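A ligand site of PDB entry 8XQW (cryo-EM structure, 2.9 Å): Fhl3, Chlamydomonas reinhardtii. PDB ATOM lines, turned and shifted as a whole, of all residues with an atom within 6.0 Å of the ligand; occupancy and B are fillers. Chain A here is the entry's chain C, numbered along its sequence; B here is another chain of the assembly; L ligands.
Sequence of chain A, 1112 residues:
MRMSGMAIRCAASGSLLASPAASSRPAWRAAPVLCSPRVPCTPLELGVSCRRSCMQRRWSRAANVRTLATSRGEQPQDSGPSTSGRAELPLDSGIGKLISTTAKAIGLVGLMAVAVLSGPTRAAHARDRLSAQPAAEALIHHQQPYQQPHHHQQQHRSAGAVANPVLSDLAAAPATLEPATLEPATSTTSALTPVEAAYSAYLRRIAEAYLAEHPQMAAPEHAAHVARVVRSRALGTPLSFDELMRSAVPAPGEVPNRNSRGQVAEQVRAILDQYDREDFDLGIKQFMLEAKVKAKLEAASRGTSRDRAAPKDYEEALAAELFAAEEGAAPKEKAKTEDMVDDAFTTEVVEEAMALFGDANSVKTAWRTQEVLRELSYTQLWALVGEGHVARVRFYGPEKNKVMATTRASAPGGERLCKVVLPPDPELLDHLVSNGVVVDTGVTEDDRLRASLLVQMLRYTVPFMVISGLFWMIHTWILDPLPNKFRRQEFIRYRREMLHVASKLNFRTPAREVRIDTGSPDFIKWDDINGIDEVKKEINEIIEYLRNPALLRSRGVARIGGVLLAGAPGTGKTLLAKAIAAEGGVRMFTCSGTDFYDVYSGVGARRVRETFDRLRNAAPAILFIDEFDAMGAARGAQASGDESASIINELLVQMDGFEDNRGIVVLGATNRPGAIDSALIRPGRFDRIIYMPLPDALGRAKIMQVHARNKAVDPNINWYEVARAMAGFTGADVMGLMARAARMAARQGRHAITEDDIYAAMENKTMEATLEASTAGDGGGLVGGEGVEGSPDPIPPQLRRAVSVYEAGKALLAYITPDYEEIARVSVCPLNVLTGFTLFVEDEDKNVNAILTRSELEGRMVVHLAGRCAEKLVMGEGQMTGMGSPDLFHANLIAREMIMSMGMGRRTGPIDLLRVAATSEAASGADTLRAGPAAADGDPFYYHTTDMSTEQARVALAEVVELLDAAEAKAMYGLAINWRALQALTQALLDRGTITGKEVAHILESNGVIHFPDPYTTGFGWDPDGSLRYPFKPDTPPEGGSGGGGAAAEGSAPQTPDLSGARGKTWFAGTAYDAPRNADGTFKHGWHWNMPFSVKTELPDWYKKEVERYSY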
ATOM      1  N   ILE A 529       7.969 -17.040 -16.139  1.00  0.00           N
ATOM      2  CA  ILE A 529       8.285 -17.308 -17.534  1.00  0.00           C
ATOM      3  C   ILE A 529       8.695 -18.761 -17.724  1.00  0.00           C
ATOM      4  O   ILE A 529       9.093 -19.450 -16.772  1.00  0.00           O
ATOM      5  CB  ILE A 529       9.392 -16.352 -18.011  1.00  0.00           C
ATOM      6  CG1 ILE A 529       9.196 -14.969 -17.387  1.00  0.00           C
ATOM      7  CG2 ILE A 529       9.414 -16.243 -19.530  1.00  0.00           C
ATOM      8  CD1 ILE A 529      10.115 -14.680 -16.220  1.00  0.00           C
ATOM      9  N   ASN A 530       8.588 -19.238 -18.965  1.00  0.00           N
ATOM     10  CA  ASN A 530       8.855 -20.626 -19.309  1.00  0.00           C
ATOM     11  C   ASN A 530      10.111 -20.728 -20.153  1.00  0.00           C
ATOM     12  O   ASN A 530      10.569 -19.771 -20.775  1.00  0.00           O
ATOM     13  CB  ASN A 530       7.666 -21.224 -20.076  1.00  0.00           C
ATOM     14  CG  ASN A 530       7.290 -20.391 -21.293  1.00  0.00           C
ATOM     15  OD1 ASN A 530       7.390 -19.153 -21.268  1.00  0.00           O
ATOM     16  ND2 ASN A 530       6.856 -21.054 -22.349  1.00  0.00           N
ATOM     17  N   ALA A 568      10.948 -12.168 -30.552  1.00  0.00           N
ATOM     18  CA  ALA A 568      10.239 -12.126 -31.849  1.00  0.00           C
ATOM     19  C   ALA A 568       8.930 -11.361 -31.695  1.00  0.00           C
ATOM     20  O   ALA A 568       8.377 -11.323 -30.583  1.00  0.00           O
ATOM     21  CB  ALA A 568       9.999 -13.538 -32.304  1.00  0.00           C
ATOM     22  N   PRO A 569       8.412 -10.734 -32.758  1.00  0.00           N
ATOM     23  CA  PRO A 569       7.131 -10.062 -32.671  1.00  0.00           C
ATOM     24  C   PRO A 569       6.155 -10.902 -31.880  1.00  0.00           C
ATOM     25  O   PRO A 569       5.750 -11.968 -32.367  1.00  0.00           O
ATOM     26  CB  PRO A 569       6.739  -9.990 -34.144  1.00  0.00           C
ATOM     27  CG  PRO A 569       8.059  -9.797 -34.852  1.00  0.00           C
ATOM     28  CD  PRO A 569       9.049 -10.630 -34.062  1.00  0.00           C
ATOM     29  N   GLY A 570       5.782 -10.445 -30.682  1.00  0.00           N
ATOM     30  CA  GLY A 570       4.763 -11.157 -29.886  1.00  0.00           C
ATOM     31  C   GLY A 570       5.369 -11.811 -28.671  1.00  0.00           C
ATOM     32  O   GLY A 570       4.683 -12.642 -28.043  1.00  0.00           O
ATOM     33  N   THR A 571       6.599 -11.453 -28.327  1.00  0.00           N
ATOM     34  CA  THR A 571       7.264 -12.119 -27.195  1.00  0.00           C
ATOM     35  C   THR A 571       6.875 -11.428 -25.905  1.00  0.00           C
ATOM     36  O   THR A 571       6.960 -12.072 -24.846  1.00  0.00           O
ATOM     37  CB  THR A 571       8.768 -12.158 -27.443  1.00  0.00           C
ATOM     38  OG1 THR A 571       8.925 -12.840 -28.682  1.00  0.00           O
ATOM     39  CG2 THR A 571       9.529 -12.937 -26.381  1.00  0.00           C
ATOM     40  N   GLY A 572       6.404 -10.186 -25.994  1.00  0.00           N
ATOM     41  CA  GLY A 572       5.944  -9.473 -24.786  1.00  0.00           C
ATOM     42  C   GLY A 572       7.018  -9.537 -23.737  1.00  0.00           C
ATOM     43  O   GLY A 572       6.767 -10.145 -22.680  1.00  0.00           O
ATOM     44  N   LYS A 573       8.163  -8.911 -24.014  1.00  0.00           N
ATOM     45  CA  LYS A 573       9.312  -9.025 -23.114  1.00  0.00           C
ATOM     46  C   LYS A 573       9.149  -8.162 -21.871  1.00  0.00           C
ATOM     47  O   LYS A 573       9.750  -8.478 -20.834  1.00  0.00           O
ATOM     48  CB  LYS A 573      10.581  -8.647 -23.863  1.00  0.00           C
ATOM     49  CG  LYS A 573      10.787  -9.433 -25.141  1.00  0.00           C
ATOM     50  CD  LYS A 573      10.903  -8.512 -26.337  1.00  0.00           C
ATOM     51  CE  LYS A 573      11.219  -9.301 -27.597  1.00  0.00           C
ATOM     52  NZ  LYS A 573      11.284  -8.428 -28.792  1.00  0.00           N
ATOM     53  N   THR A 574       8.361  -7.091 -21.960  1.00  0.00           N
ATOM     54  CA  THR A 574       8.033  -6.272 -20.803  1.00  0.00           C
ATOM     55  C   THR A 574       7.734  -7.144 -19.586  1.00  0.00           C
ATOM     56  O   THR A 574       8.246  -6.871 -18.483  1.00  0.00           O
ATOM     57  CB  THR A 574       6.808  -5.394 -21.108  1.00  0.00           C
ATOM     58  OG1 THR A 574       5.619  -6.126 -20.785  1.00  0.00           O
ATOM     59  CG2 THR A 574       6.777  -5.023 -22.579  1.00  0.00           C
ATOM     60  N   LEU A 575       6.925  -8.177 -19.772  1.00  0.00           N
ATOM     61  CA  LEU A 575       6.606  -9.114 -18.705  1.00  0.00           C
ATOM     62  C   LEU A 575       7.845  -9.501 -17.924  1.00  0.00           C
ATOM     63  O   LEU A 575       7.942  -9.200 -16.721  1.00  0.00           O
ATOM     64  CB  LEU A 575       5.930 -10.350 -19.317  1.00  0.00           C
ATOM     65  CG  LEU A 575       5.141 -11.365 -18.491  1.00  0.00           C
ATOM     66  CD1 LEU A 575       6.033 -12.427 -17.863  1.00  0.00           C
ATOM     67  CD2 LEU A 575       4.336 -10.643 -17.447  1.00  0.00           C
ATOM     68  N   ASP A 626      11.107  -0.565 -24.730  1.00  0.00           N
ATOM     69  CA  ASP A 626      10.561  -1.266 -25.881  1.00  0.00           C
ATOM     70  C   ASP A 626      10.805  -0.450 -27.142  1.00  0.00           C
ATOM     71  O   ASP A 626      11.232   0.713 -27.088  1.00  0.00           O
ATOM     72  CB  ASP A 626       9.066  -1.515 -25.680  1.00  0.00           C
ATOM     73  CG  ASP A 626       8.638  -2.914 -26.132  1.00  0.00           C
ATOM     74  OD1 ASP A 626       9.326  -3.894 -25.776  1.00  0.00           O
ATOM     75  OD2 ASP A 626       7.624  -3.028 -26.846  1.00  0.00           O
ATOM     76  N   GLU A 627      10.559  -1.065 -28.293  1.00  0.00           N
ATOM     77  CA  GLU A 627      10.720  -0.399 -29.583  1.00  0.00           C
ATOM     78  C   GLU A 627      12.156   0.098 -29.777  1.00  0.00           C
ATOM     79  O   GLU A 627      12.394   1.175 -30.328  1.00  0.00           O
ATOM     80  CB  GLU A 627       9.724   0.756 -29.736  1.00  0.00           C
ATOM     81  CG  GLU A 627       8.472   0.458 -30.582  1.00  0.00           C
ATOM     82  CD  GLU A 627       8.781  -0.031 -31.986  1.00  0.00           C
ATOM     83  OE1 GLU A 627       7.826  -0.421 -32.696  1.00  0.00           O
ATOM     84  OE2 GLU A 627       9.950   0.001 -32.414  1.00  0.00           O
ATOM     85  N   MET A 692      14.511 -14.486 -25.500  1.00  0.00           N
ATOM     86  CA  MET A 692      13.255 -14.986 -24.950  1.00  0.00           C
ATOM     87  C   MET A 692      12.530 -15.784 -26.019  1.00  0.00           C
ATOM     88  O   MET A 692      12.076 -15.201 -27.017  1.00  0.00           O
ATOM     89  CB  MET A 692      12.383 -13.820 -24.468  1.00  0.00           C
ATOM     90  CG  MET A 692      11.663 -14.083 -23.151  1.00  0.00           C
ATOM     91  SD  MET A 692      10.762 -12.628 -22.593  1.00  0.00           S
ATOM     92  CE  MET A 692       9.444 -13.380 -21.646  1.00  0.00           C
ATOM     93  N   ILE A 703      -0.452 -19.878 -20.162  1.00  0.00           N
ATOM     94  CA  ILE A 703      -0.853 -18.556 -20.640  1.00  0.00           C
ATOM     95  C   ILE A 703      -2.370 -18.453 -20.726  1.00  0.00           C
ATOM     96  O   ILE A 703      -2.962 -17.450 -20.334  1.00  0.00           O
ATOM     97  CB  ILE A 703      -0.207 -18.237 -21.992  1.00  0.00           C
ATOM     98  CG1 ILE A 703       1.269 -17.917 -21.821  1.00  0.00           C
ATOM     99  CG2 ILE A 703      -0.901 -17.075 -22.656  1.00  0.00           C
ATOM    100  CD1 ILE A 703       1.892 -17.323 -23.046  1.00  0.00           C
ATOM    101  N   VAL A 706      -4.647 -18.185 -17.521  1.00  0.00           N
ATOM    102  CA  VAL A 706      -4.777 -16.920 -16.827  1.00  0.00           C
ATOM    103  C   VAL A 706      -5.660 -15.953 -17.602  1.00  0.00           C
ATOM    104  O   VAL A 706      -6.265 -15.053 -17.009  1.00  0.00           O
ATOM    105  CB  VAL A 706      -3.388 -16.310 -16.548  1.00  0.00           C
ATOM    106  CG1 VAL A 706      -2.450 -17.394 -16.056  1.00  0.00           C
ATOM    107  CG2 VAL A 706      -2.836 -15.632 -17.786  1.00  0.00           C
ATOM    108  N   HIS A 707      -5.756 -16.105 -18.912  1.00  0.00           N
ATOM    109  CA  HIS A 707      -6.730 -15.349 -19.681  1.00  0.00           C
ATOM    110  C   HIS A 707      -8.151 -15.829 -19.424  1.00  0.00           C
ATOM    111  O   HIS A 707      -9.091 -15.309 -20.037  1.00  0.00           O
ATOM    112  CB  HIS A 707      -6.425 -15.435 -21.176  1.00  0.00           C
ATOM    113  CG  HIS A 707      -5.654 -14.259 -21.698  1.00  0.00           C
ATOM    114  ND1 HIS A 707      -4.493 -14.403 -22.423  1.00  0.00           N
ATOM    115  CD2 HIS A 707      -5.903 -12.939 -21.633  1.00  0.00           C
ATOM    116  CE1 HIS A 707      -4.046 -13.209 -22.756  1.00  0.00           C
ATOM    117  NE2 HIS A 707      -4.883 -12.296 -22.297  1.00  0.00           N
ATOM    118  N   THR A 730       2.400 -17.384 -30.214  1.00  0.00           N
ATOM    119  CA  THR A 730       2.938 -16.565 -29.148  1.00  0.00           C
ATOM    120  C   THR A 730       1.822 -16.237 -28.167  1.00  0.00           C
ATOM    121  O   THR A 730       0.709 -16.742 -28.271  1.00  0.00           O
ATOM    122  CB  THR A 730       3.572 -15.298 -29.714  1.00  0.00           C
ATOM    123  OG1 THR A 730       2.589 -14.254 -29.702  1.00  0.00           O
ATOM    124  CG2 THR A 730       4.027 -15.539 -31.126  1.00  0.00           C
ATOM    125  N   GLY A 731       2.127 -15.370 -27.205  1.00  0.00           N
ATOM    126  CA  GLY A 731       1.095 -14.947 -26.273  1.00  0.00           C
ATOM    127  C   GLY A 731       0.012 -14.125 -26.937  1.00  0.00           C
ATOM    128  O   GLY A 731      -1.175 -14.253 -26.615  1.00  0.00           O
ATOM    129  N   ALA A 732       0.410 -13.246 -27.863  1.00  0.00           N
ATOM    130  CA  ALA A 732      -0.559 -12.453 -28.597  1.00  0.00           C
ATOM    131  C   ALA A 732      -1.531 -13.341 -29.356  1.00  0.00           C
ATOM    132  O   ALA A 732      -2.739 -13.078 -29.390  1.00  0.00           O
ATOM    133  CB  ALA A 732       0.152 -11.505 -29.559  1.00  0.00           C
ATOM    134  N   MET A 735      -4.100 -14.767 -26.875  1.00  0.00           N
ATOM    135  CA  MET A 735      -5.138 -13.829 -26.435  1.00  0.00           C
ATOM    136  C   MET A 735      -6.108 -13.498 -27.565  1.00  0.00           C
ATOM    137  O   MET A 735      -7.326 -13.412 -27.341  1.00  0.00           O
ATOM    138  CB  MET A 735      -4.497 -12.557 -25.856  1.00  0.00           C
ATOM    139  CG  MET A 735      -3.692 -11.695 -26.801  1.00  0.00           C
ATOM    140  SD  MET A 735      -4.689 -10.574 -27.805  1.00  0.00           S
ATOM    141  CE  MET A 735      -3.488  -9.292 -28.182  1.00  0.00           C
ATOM    142  N   LEU B2300       1.868   1.121 -36.644  1.00  0.00           N
ATOM    143  CA  LEU B2300       1.627  -0.017 -35.776  1.00  0.00           C
ATOM    144  C   LEU B2300       1.441   0.434 -34.343  1.00  0.00           C
ATOM    145  O   LEU B2300       0.539  -0.044 -33.635  1.00  0.00           O
ATOM    146  CB  LEU B2300       2.783  -1.009 -35.898  1.00  0.00           C
ATOM    147  CG  LEU B2300       2.546  -2.499 -35.672  1.00  0.00           C
ATOM    148  CD1 LEU B2300       2.132  -2.822 -34.244  1.00  0.00           C
ATOM    149  CD2 LEU B2300       1.500  -2.976 -36.657  1.00  0.00           C
ATOM    150  N   ASP B2304      -2.033   0.053 -32.206  1.00  0.00           N
ATOM    151  CA  ASP B2304      -2.078  -0.643 -30.934  1.00  0.00           C
ATOM    152  C   ASP B2304      -2.433   0.285 -29.791  1.00  0.00           C
ATOM    153  O   ASP B2304      -2.827  -0.183 -28.713  1.00  0.00           O
ATOM    154  CB  ASP B2304      -0.749  -1.335 -30.665  1.00  0.00           C
ATOM    155  CG  ASP B2304      -0.844  -2.373 -29.553  1.00  0.00           C
ATOM    156  OD1 ASP B2304      -0.870  -1.985 -28.377  1.00  0.00           O
ATOM    157  OD2 ASP B2304      -0.898  -3.577 -29.879  1.00  0.00           O
ATOM    158  N   ARG B2307      -6.629   0.581 -27.621  1.00  0.00           N
ATOM    159  CA  ARG B2307      -7.415  -0.366 -26.840  1.00  0.00           C
ATOM    160  C   ARG B2307      -7.211  -0.098 -25.365  1.00  0.00           C
ATOM    161  O   ARG B2307      -7.700  -0.874 -24.536  1.00  0.00           O
ATOM    162  CB  ARG B2307      -7.060  -1.806 -27.172  1.00  0.00           C
ATOM    163  CG  ARG B2307      -5.697  -2.241 -26.727  1.00  0.00           C
ATOM    164  CD  ARG B2307      -5.602  -3.746 -26.736  1.00  0.00           C
ATOM    165  NE  ARG B2307      -4.220  -4.210 -26.604  1.00  0.00           N
ATOM    166  CZ  ARG B2307      -3.465  -4.581 -27.633  1.00  0.00           C
ATOM    167  NH1 ARG B2307      -3.952  -4.545 -28.859  1.00  0.00           N
ATOM    168  NH2 ARG B2307      -2.224  -4.987 -27.419  1.00  0.00           N
ATOM    169  N   ARG B2333      -4.731  -5.930 -33.434  1.00  0.00           N
ATOM    170  CA  ARG B2333      -4.672  -4.700 -34.205  1.00  0.00           C
ATOM    171  C   ARG B2333      -5.815  -4.574 -35.210  1.00  0.00           C
ATOM    172  O   ARG B2333      -6.624  -3.659 -35.087  1.00  0.00           O
ATOM    173  CB  ARG B2333      -3.312  -4.621 -34.918  1.00  0.00           C
ATOM    174  CG  ARG B2333      -2.154  -4.836 -33.979  1.00  0.00           C
ATOM    175  CD  ARG B2333      -0.844  -4.921 -34.727  1.00  0.00           C
ATOM    176  NE  ARG B2333      -0.078  -6.094 -34.333  1.00  0.00           N
ATOM    177  CZ  ARG B2333       0.620  -6.170 -33.209  1.00  0.00           C
ATOM    178  NH1 ARG B2333       0.637  -5.158 -32.359  1.00  0.00           N
ATOM    179  NH2 ARG B2333       1.303  -7.280 -32.931  1.00  0.00           N
HETATM  180  P1  LIG L   1       5.760  -6.301 -30.777  1.00  0.00           P
HETATM  181  O1  LIG L   1       4.983  -6.290 -32.054  1.00  0.00           O
HETATM  182  O2  LIG L   1       6.921  -7.349 -30.889  1.00  0.00           O
HETATM  183  O3  LIG L   1       6.357  -4.869 -30.517  1.00  0.00           O
HETATM  184  P2  LIG L   1       5.750  -7.265 -28.240  1.00  0.00           P
HETATM  185  O4  LIG L   1       6.635  -6.171 -27.768  1.00  0.00           O
HETATM  186  O5  LIG L   1       6.630  -8.450 -28.746  1.00  0.00           O
HETATM  187  N1  LIG L   1       4.762  -6.724 -29.486  1.00  0.00           N
HETATM  188  P3  LIG L   1       3.430  -7.115 -26.821  1.00  0.00           P
HETATM  189  O6  LIG L   1       2.822  -6.707 -28.098  1.00  0.00           O
HETATM  190  O7  LIG L   1       3.646  -5.980 -25.815  1.00  0.00           O
HETATM  191  O8  LIG L   1       4.861  -7.754 -27.053  1.00  0.00           O
HETATM  192  O9  LIG L   1       2.572  -8.279 -26.191  1.00  0.00           O
HETATM  193  C1  LIG L   1       1.543  -8.963 -26.933  1.00  0.00           C
HETATM  194  C2  LIG L   1       0.733  -9.797 -25.970  1.00  0.00           C
HETATM  195  O10 LIG L   1       1.468 -10.991 -25.632  1.00  0.00           O
HETATM  196  C3  LIG L   1       0.448  -9.141 -24.621  1.00  0.00           C
HETATM  197  O11 LIG L   1      -0.773  -8.414 -24.680  1.00  0.00           O
HETATM  198  C4  LIG L   1       0.359 -10.333 -23.651  1.00  0.00           C
HETATM  199  O12 LIG L   1      -0.974 -10.593 -23.232  1.00  0.00           O
HETATM  200  C5  LIG L   1       0.891 -11.520 -24.460  1.00  0.00           C
HETATM  201  N2  LIG L   1       1.898 -12.324 -23.780  1.00  0.00           N
HETATM  202  C6  LIG L   1       3.164 -12.589 -24.200  1.00  0.00           C
HETATM  203  N3  LIG L   1       3.857 -13.356 -23.390  1.00  0.00           N
HETATM  204  C7  LIG L   1       2.971 -13.606 -22.360  1.00  0.00           C
HETATM  205  C8  LIG L   1       3.094 -14.368 -21.172  1.00  0.00           C
HETATM  206  N4  LIG L   1       4.198 -15.015 -20.817  1.00  0.00           N
HETATM  207  N5  LIG L   1       2.013 -14.419 -20.356  1.00  0.00           N
HETATM  208  C9  LIG L   1       0.904 -13.766 -20.704  1.00  0.00           C
HETATM  209  N6  LIG L   1       0.679 -13.017 -21.790  1.00  0.00           N
HETATM  210  C10 LIG L   1       1.749 -12.984 -22.583  1.00  0.00           C
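N of Thr 571 lies within hydrogen-bond range of O5 of the ligand (3.0 Å).
An oxygen (O10) of the ligand sits at hydrogen-bond distance from the backbone NH of Ala 732 (3.3 Å).
NH2 of Arg 2333 of chain B lies within salt-bridge range of O1 of the ligand, 3.9 Å away.
N of Gly 572 sits close to O8 of the ligand.
The backbone NH of Gly 570 lies within hydrogen-bond range of an oxygen (O5) of the ligand (2.9 Å).
O of Gly 570 lies within hydrogen-bond range of OG1 of Thr 730 (3.1 Å).
The side-chain carboxylate of Asp 2304 of chain B lies within salt-bridge range of the guanidinium group of Arg 2333 of chain B, at 3.3 Å.
OG1 of Thr 730 lies within hydrogen-bond range of N of Ala 732, at 3.0 Å.
The backbone carbonyl oxygen of Ala 568 is in hydrogen-bond range of the side-chain hydroxyl of Thr 571 (2.5 Å).
OD2 of Asp 626 lies close to O4 of the ligand (3.4 Å).
Ala 568 touches the ligand.
CA of Pro 569 touches O2 of the ligand, 3.3 Å away.
CD1 of Ile 703 touches C8 of the ligand, 3.7 Å away.
C of Gly 731 touches O10 of the ligand, 3.7 Å away.
Hydrophobic or aromatic side chains that line the ligand: Ile 703 and Ala 732.
Within 4 Å of the ligand: Ala 568, Pro 569, Gly 570, Thr 571, Gly 572, Asp 626, Ile 703, Gly 731, Ala 732 and Arg 2333 of chain B.
The nearest printed residue that does not touch the ligand is His 707 (4.1 Å).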
